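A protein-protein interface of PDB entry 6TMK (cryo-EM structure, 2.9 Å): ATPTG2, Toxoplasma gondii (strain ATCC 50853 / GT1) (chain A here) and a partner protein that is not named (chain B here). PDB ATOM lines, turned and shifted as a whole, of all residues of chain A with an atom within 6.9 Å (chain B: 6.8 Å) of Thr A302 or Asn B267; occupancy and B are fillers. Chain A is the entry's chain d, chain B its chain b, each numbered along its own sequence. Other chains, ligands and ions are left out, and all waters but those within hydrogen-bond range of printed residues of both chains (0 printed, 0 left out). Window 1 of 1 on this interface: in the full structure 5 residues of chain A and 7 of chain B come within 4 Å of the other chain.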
ATOM      1  N   ALA A 297      -9.325  22.944 -24.171  1.00  0.00           N
ATOM      2  CA  ALA A 297      -8.721  23.877 -23.227  1.00  0.00           C
ATOM      3  C   ALA A 297      -8.608  23.283 -21.824  1.00  0.00           C
ATOM      4  O   ALA A 297      -8.808  23.971 -20.825  1.00  0.00           O
ATOM      5  CB  ALA A 297      -9.514  25.172 -23.181  1.00  0.00           C
ATOM      6  N   ARG A 298      -8.268  21.996 -21.741  1.00  0.00           N
ATOM      7  CA  ARG A 298      -8.159  21.329 -20.449  1.00  0.00           C
ATOM      8  C   ARG A 298      -7.049  21.919 -19.596  1.00  0.00           C
ATOM      9  O   ARG A 298      -7.144  21.924 -18.366  1.00  0.00           O
ATOM     10  CB  ARG A 298      -7.909  19.844 -20.684  1.00  0.00           C
ATOM     11  CG  ARG A 298      -8.075  18.943 -19.492  1.00  0.00           C
ATOM     12  CD  ARG A 298      -7.450  17.612 -19.792  1.00  0.00           C
ATOM     13  NE  ARG A 298      -8.009  17.049 -21.011  1.00  0.00           N
ATOM     14  CZ  ARG A 298      -9.220  16.511 -21.096  1.00  0.00           C
ATOM     15  NH1 ARG A 298      -9.996  16.443 -20.028  1.00  0.00           N
ATOM     16  NH2 ARG A 298      -9.653  16.040 -22.252  1.00  0.00           N
ATOM     17  N   MET A 299      -5.995  22.421 -20.233  1.00  0.00           N
ATOM     18  CA  MET A 299      -4.874  23.010 -19.512  1.00  0.00           C
ATOM     19  C   MET A 299      -5.305  24.174 -18.631  1.00  0.00           C
ATOM     20  O   MET A 299      -4.652  24.466 -17.624  1.00  0.00           O
ATOM     21  CB  MET A 299      -3.827  23.469 -20.512  1.00  0.00           C
ATOM     22  CG  MET A 299      -2.485  23.763 -19.929  1.00  0.00           C
ATOM     23  SD  MET A 299      -1.482  24.666 -21.108  1.00  0.00           S
ATOM     24  CE  MET A 299       0.121  24.366 -20.406  1.00  0.00           C
ATOM     25  N   MET A 300      -6.402  24.837 -18.981  1.00  0.00           N
ATOM     26  CA  MET A 300      -6.860  26.009 -18.255  1.00  0.00           C
ATOM     27  C   MET A 300      -7.624  25.668 -16.989  1.00  0.00           C
ATOM     28  O   MET A 300      -7.848  26.556 -16.162  1.00  0.00           O
ATOM     29  CB  MET A 300      -7.739  26.843 -19.173  1.00  0.00           C
ATOM     30  CG  MET A 300      -6.963  27.550 -20.253  1.00  0.00           C
ATOM     31  SD  MET A 300      -8.018  28.172 -21.565  1.00  0.00           S
ATOM     32  CE  MET A 300      -9.011  29.290 -20.613  1.00  0.00           C
ATOM     33  N   PHE A 301      -8.043  24.419 -16.829  1.00  0.00           N
ATOM     34  CA  PHE A 301      -8.753  23.955 -15.648  1.00  0.00           C
ATOM     35  C   PHE A 301      -7.850  23.148 -14.722  1.00  0.00           C
ATOM     36  O   PHE A 301      -8.314  22.217 -14.060  1.00  0.00           O
ATOM     37  CB  PHE A 301      -9.968  23.148 -16.085  1.00  0.00           C
ATOM     38  CG  PHE A 301     -10.815  23.858 -17.089  1.00  0.00           C
ATOM     39  CD1 PHE A 301     -11.723  24.812 -16.688  1.00  0.00           C
ATOM     40  CD2 PHE A 301     -10.679  23.603 -18.436  1.00  0.00           C
ATOM     41  CE1 PHE A 301     -12.487  25.479 -17.606  1.00  0.00           C
ATOM     42  CE2 PHE A 301     -11.443  24.269 -19.353  1.00  0.00           C
ATOM     43  CZ  PHE A 301     -12.347  25.209 -18.938  1.00  0.00           C
ATOM     44  N   THR A 302      -6.569  23.506 -14.647  1.00  0.00           N
ATOM     45  CA  THR A 302      -5.585  22.747 -13.896  1.00  0.00           C
ATOM     46  C   THR A 302      -4.628  23.681 -13.175  1.00  0.00           C
ATOM     47  O   THR A 302      -4.252  24.727 -13.709  1.00  0.00           O
ATOM     48  CB  THR A 302      -4.766  21.829 -14.811  1.00  0.00           C
ATOM     49  OG1 THR A 302      -3.996  22.617 -15.722  1.00  0.00           O
ATOM     50  CG2 THR A 302      -5.665  20.928 -15.597  1.00  0.00           C
ATOM     51  N   ASP A 303      -4.246  23.303 -11.957  1.00  0.00           N
ATOM     52  CA  ASP A 303      -3.174  24.005 -11.267  1.00  0.00           C
ATOM     53  C   ASP A 303      -1.798  23.548 -11.740  1.00  0.00           C
ATOM     54  O   ASP A 303      -0.842  24.325 -11.691  1.00  0.00           O
ATOM     55  CB  ASP A 303      -3.320  23.805  -9.760  1.00  0.00           C
ATOM     56  CG  ASP A 303      -4.134  24.899  -9.102  1.00  0.00           C
ATOM     57  OD1 ASP A 303      -3.991  26.073  -9.501  1.00  0.00           O
ATOM     58  OD2 ASP A 303      -4.920  24.585  -8.184  1.00  0.00           O
ATOM     59  N   VAL A 304      -1.680  22.301 -12.192  1.00  0.00           N
ATOM     60  CA  VAL A 304      -0.441  21.761 -12.731  1.00  0.00           C
ATOM     61  C   VAL A 304      -0.802  20.881 -13.917  1.00  0.00           C
ATOM     62  O   VAL A 304      -1.884  20.292 -13.970  1.00  0.00           O
ATOM     63  CB  VAL A 304       0.380  20.960 -11.691  1.00  0.00           C
ATOM     64  CG1 VAL A 304       1.052  21.870 -10.731  1.00  0.00           C
ATOM     65  CG2 VAL A 304      -0.503  20.031 -10.926  1.00  0.00           C
ATOM     66  N   PHE A 305       0.126  20.776 -14.861  1.00  0.00           N
ATOM     67  CA  PHE A 305      -0.105  20.012 -16.076  1.00  0.00           C
ATOM     68  C   PHE A 305       1.216  19.400 -16.509  1.00  0.00           C
ATOM     69  O   PHE A 305       2.204  20.119 -16.677  1.00  0.00           O
ATOM     70  CB  PHE A 305      -0.682  20.898 -17.182  1.00  0.00           C
ATOM     71  CG  PHE A 305      -1.417  20.151 -18.244  1.00  0.00           C
ATOM     72  CD1 PHE A 305      -0.788  19.778 -19.409  1.00  0.00           C
ATOM     73  CD2 PHE A 305      -2.755  19.855 -18.093  1.00  0.00           C
ATOM     74  CE1 PHE A 305      -1.465  19.105 -20.379  1.00  0.00           C
ATOM     75  CE2 PHE A 305      -3.440  19.183 -19.070  1.00  0.00           C
ATOM     76  CZ  PHE A 305      -2.799  18.813 -20.213  1.00  0.00           C
ATOM     77  N   ASN B 262       3.950  25.897 -12.987  1.00  0.00           N
ATOM     78  CA  ASN B 262       2.540  25.575 -12.820  1.00  0.00           C
ATOM     79  C   ASN B 262       1.738  26.392 -13.822  1.00  0.00           C
ATOM     80  O   ASN B 262       2.282  27.220 -14.558  1.00  0.00           O
ATOM     81  CB  ASN B 262       2.089  25.821 -11.385  1.00  0.00           C
ATOM     82  CG  ASN B 262       2.435  27.196 -10.887  1.00  0.00           C
ATOM     83  OD1 ASN B 262       2.196  28.199 -11.553  1.00  0.00           O
ATOM     84  ND2 ASN B 262       3.003  27.249  -9.698  1.00  0.00           N
ATOM     85  N   THR B 263       0.432  26.139 -13.848  1.00  0.00           N
ATOM     86  CA  THR B 263      -0.501  26.814 -14.735  1.00  0.00           C
ATOM     87  C   THR B 263      -1.386  27.796 -13.977  1.00  0.00           C
ATOM     88  O   THR B 263      -2.499  28.100 -14.404  1.00  0.00           O
ATOM     89  CB  THR B 263      -1.355  25.774 -15.459  1.00  0.00           C
ATOM     90  OG1 THR B 263      -0.525  24.694 -15.893  1.00  0.00           O
ATOM     91  CG2 THR B 263      -2.046  26.374 -16.666  1.00  0.00           C
ATOM     92  N   VAL B 264      -0.901  28.292 -12.840  1.00  0.00           N
ATOM     93  CA  VAL B 264      -1.743  29.106 -11.972  1.00  0.00           C
ATOM     94  C   VAL B 264      -2.072  30.441 -12.624  1.00  0.00           C
ATOM     95  O   VAL B 264      -3.219  30.898 -12.583  1.00  0.00           O
ATOM     96  CB  VAL B 264      -1.062  29.291 -10.605  1.00  0.00           C
ATOM     97  CG1 VAL B 264      -1.657  30.455  -9.867  1.00  0.00           C
ATOM     98  CG2 VAL B 264      -1.199  28.042  -9.791  1.00  0.00           C
ATOM     99  N   LEU B 265      -1.083  31.088 -13.235  1.00  0.00           N
ATOM    100  CA  LEU B 265      -1.298  32.390 -13.846  1.00  0.00           C
ATOM    101  C   LEU B 265      -1.898  32.300 -15.241  1.00  0.00           C
ATOM    102  O   LEU B 265      -2.011  33.328 -15.913  1.00  0.00           O
ATOM    103  CB  LEU B 265       0.017  33.170 -13.890  1.00  0.00           C
ATOM    104  CG  LEU B 265       0.758  33.287 -12.559  1.00  0.00           C
ATOM    105  CD1 LEU B 265       2.058  34.010 -12.755  1.00  0.00           C
ATOM    106  CD2 LEU B 265      -0.098  34.013 -11.555  1.00  0.00           C
ATOM    107  N   SER B 266      -2.293  31.107 -15.681  1.00  0.00           N
ATOM    108  CA  SER B 266      -2.898  30.907 -16.989  1.00  0.00           C
ATOM    109  C   SER B 266      -4.229  30.187 -16.843  1.00  0.00           C
ATOM    110  O   SER B 266      -4.681  29.500 -17.759  1.00  0.00           O
ATOM    111  CB  SER B 266      -1.963  30.111 -17.894  1.00  0.00           C
ATOM    112  OG  SER B 266      -0.752  30.801 -18.118  1.00  0.00           O
ATOM    113  N   ASN B 267      -4.863  30.356 -15.697  1.00  0.00           N
ATOM    114  CA  ASN B 267      -6.004  29.564 -15.274  1.00  0.00           C
ATOM    115  C   ASN B 267      -7.325  30.252 -15.571  1.00  0.00           C
ATOM    116  O   ASN B 267      -7.434  31.481 -15.574  1.00  0.00           O
ATOM    117  CB  ASN B 267      -5.931  29.239 -13.782  1.00  0.00           C
ATOM    118  CG  ASN B 267      -5.392  27.865 -13.514  1.00  0.00           C
ATOM    119  OD1 ASN B 267      -5.058  27.121 -14.434  1.00  0.00           O
ATOM    120  ND2 ASN B 267      -5.311  27.512 -12.248  1.00  0.00           N
ATOM    121  N   ALA B 268      -8.344  29.423 -15.784  1.00  0.00           N
ATOM    122  CA  ALA B 268      -9.703  29.928 -15.871  1.00  0.00           C
ATOM    123  C   ALA B 268     -10.117  30.539 -14.545  1.00  0.00           C
ATOM    124  O   ALA B 268     -10.801  31.564 -14.517  1.00  0.00           O
ATOM    125  CB  ALA B 268     -10.660  28.811 -16.277  1.00  0.00           C
ATOM    126  N   TRP B 269      -9.699  29.936 -13.433  1.00  0.00           N
ATOM    127  CA  TRP B 269      -9.956  30.539 -12.134  1.00  0.00           C
ATOM    128  C   TRP B 269      -9.312  31.911 -12.057  1.00  0.00           C
ATOM    129  O   TRP B 269      -9.941  32.883 -11.635  1.00  0.00           O
ATOM    130  CB  TRP B 269      -9.410  29.673 -11.007  1.00  0.00           C
ATOM    131  CG  TRP B 269      -9.601  30.320  -9.682  1.00  0.00           C
ATOM    132  CD1 TRP B 269      -8.729  31.137  -9.035  1.00  0.00           C
ATOM    133  CD2 TRP B 269     -10.743  30.204  -8.834  1.00  0.00           C
ATOM    134  NE1 TRP B 269      -9.259  31.546  -7.848  1.00  0.00           N
ATOM    135  CE2 TRP B 269     -10.495  30.983  -7.696  1.00  0.00           C
ATOM    136  CE3 TRP B 269     -11.953  29.519  -8.928  1.00  0.00           C
ATOM    137  CZ2 TRP B 269     -11.409  31.094  -6.661  1.00  0.00           C
ATOM    138  CZ3 TRP B 269     -12.855  29.634  -7.903  1.00  0.00           C
ATOM    139  CH2 TRP B 269     -12.581  30.412  -6.784  1.00  0.00           C
ATOM    140  N   PHE B 270      -8.046  32.007 -12.458  1.00  0.00           N
ATOM    141  CA  PHE B 270      -7.374  33.294 -12.467  1.00  0.00           C
ATOM    142  C   PHE B 270      -8.189  34.317 -13.247  1.00  0.00           C
ATOM    143  O   PHE B 270      -8.706  35.276 -12.670  1.00  0.00           O
ATOM    144  CB  PHE B 270      -5.976  33.134 -13.058  1.00  0.00           C
ATOM    145  CG  PHE B 270      -5.148  34.367 -12.997  1.00  0.00           C
ATOM    146  CD1 PHE B 270      -4.591  34.784 -11.813  1.00  0.00           C
ATOM    147  CD2 PHE B 270      -4.927  35.117 -14.131  1.00  0.00           C
ATOM    148  CE1 PHE B 270      -3.836  35.919 -11.759  1.00  0.00           C
ATOM    149  CE2 PHE B 270      -4.172  36.253 -14.082  1.00  0.00           C
ATOM    150  CZ  PHE B 270      -3.626  36.657 -12.899  1.00  0.00           C
ATOM    151  N   TYR B 271      -8.406  34.058 -14.538  1.00  0.00           N
ATOM    152  CA  TYR B 271      -9.051  35.035 -15.404  1.00  0.00           C
ATOM    153  C   TYR B 271     -10.505  35.310 -15.039  1.00  0.00           C
ATOM    154  O   TYR B 271     -11.018  36.373 -15.393  1.00  0.00           O
ATOM    155  CB  TYR B 271      -8.976  34.569 -16.852  1.00  0.00           C
ATOM    156  CG  TYR B 271      -7.584  34.497 -17.416  1.00  0.00           C
ATOM    157  CD1 TYR B 271      -6.737  35.588 -17.375  1.00  0.00           C
ATOM    158  CD2 TYR B 271      -7.117  33.335 -18.003  1.00  0.00           C
ATOM    159  CE1 TYR B 271      -5.477  35.521 -17.889  1.00  0.00           C
ATOM    160  CE2 TYR B 271      -5.854  33.264 -18.519  1.00  0.00           C
ATOM    161  CZ  TYR B 271      -5.037  34.363 -18.460  1.00  0.00           C
ATOM    162  OH  TYR B 271      -3.771  34.309 -18.974  1.00  0.00           O
ATOM    163  N   SER B 272     -11.182  34.395 -14.347  1.00  0.00           N
ATOM    164  CA  SER B 272     -12.589  34.575 -14.017  1.00  0.00           C
ATOM    165  C   SER B 272     -12.812  35.204 -12.653  1.00  0.00           C
ATOM    166  O   SER B 272     -13.784  35.945 -12.479  1.00  0.00           O
ATOM    167  CB  SER B 272     -13.321  33.236 -14.071  1.00  0.00           C
ATOM    168  OG  SER B 272     -13.281  32.684 -15.367  1.00  0.00           O
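The backbone NH (N) of Ala B268 is in hydrogen-bond range of the backbone carbonyl oxygen (O) of Met A300 (2.9 Å).
OD1 of Asp A303 is in hydrogen-bond range of ND2 of Asn B267, at 3.4 Å.
The side-chain amide oxygen (OD1) of Asn B267 sits close to the backbone carbonyl oxygen (O) of Met A300 (3.3 Å).
The backbone NH of Thr B263 lies within hydrogen-bond range of the backbone carbonyl oxygen of Asp A303, at 3.1 Å.
OD1 of Asn B267 lies close to O of Thr A302 (2.6 Å).
The backbone carbonyl oxygen (O) of Thr B263 sits close to the side-chain amide oxygen (OD1) of Asn B267 (2.7 Å).
O of Met A299 lies within hydrogen-bond range of OG1 of Thr A302 (2.7 Å).
The side-chain hydroxyl of Ser B272 sits at hydrogen-bond distance from the backbone carbonyl oxygen of Ala B268 (2.9 Å).
The backbone NH (N) of Val B264 is in hydrogen-bond range of the side-chain amide oxygen (OD1) of Asn B262, at 3.4 Å.
CG2 of Thr B263 touches O of Met A299, 3.4 Å away.
Met A300 touches Ser B266 (CG to O, 3.9 Å).
Thr B263 touches Thr A302.
Asp A303 touches Asn B262.
Asp A303 touches Val B264 (OD1 to CG2, 3.4 Å).
Thr A302 touches two residues of chain B.
Of the printed residues of chain A, Asn B267 touches Met A300 (3.3 Å), Thr A302 (2.6 Å) and Asp A303 (3.4 Å).
Of the printed residues of chain B, Met A299 touches Thr B263 (3.4 Å).
Of the printed residues of chain A, Val B264 touches Asp A303.
Of the printed residues of chain A, Ala B268 touches Met A300 (2.9 Å).
Of the printed residues of chain B, Met A300 touches Ser B266, Asn B267 and Ala B268.
Printed residues of chain B within 4 Å of Asp A303: Asn B262 (3.3 Å), Thr B263 (3.1 Å), Val B264 (3.4 Å) and Asn B267 (3.4 Å).
Tyr B271 touches none of the printed residues of chain A.
Phe A301 touches none of the printed residues of chain B.
The nearest residue of chain A that does not touch Asn B267 is Met A299 (4.2 Å).
Of the 11 printed residues of chain B, 6 touch a printed residue of chain A.
Hydrophobic or aromatic side chains of chain B within 4 Å of the printed part of chain A: Val B264 and Ala B268.
Hydrophobic or aromatic side chains of chain A within 4 Å of the printed part of chain B: Met A300.
Among the printed residues, 10 pairs touch across the chains.
Among the printed residues, no Asp or Glu carboxylate lies within 4 Å of a Lys or Arg side-chain nitrogen of the other chain.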
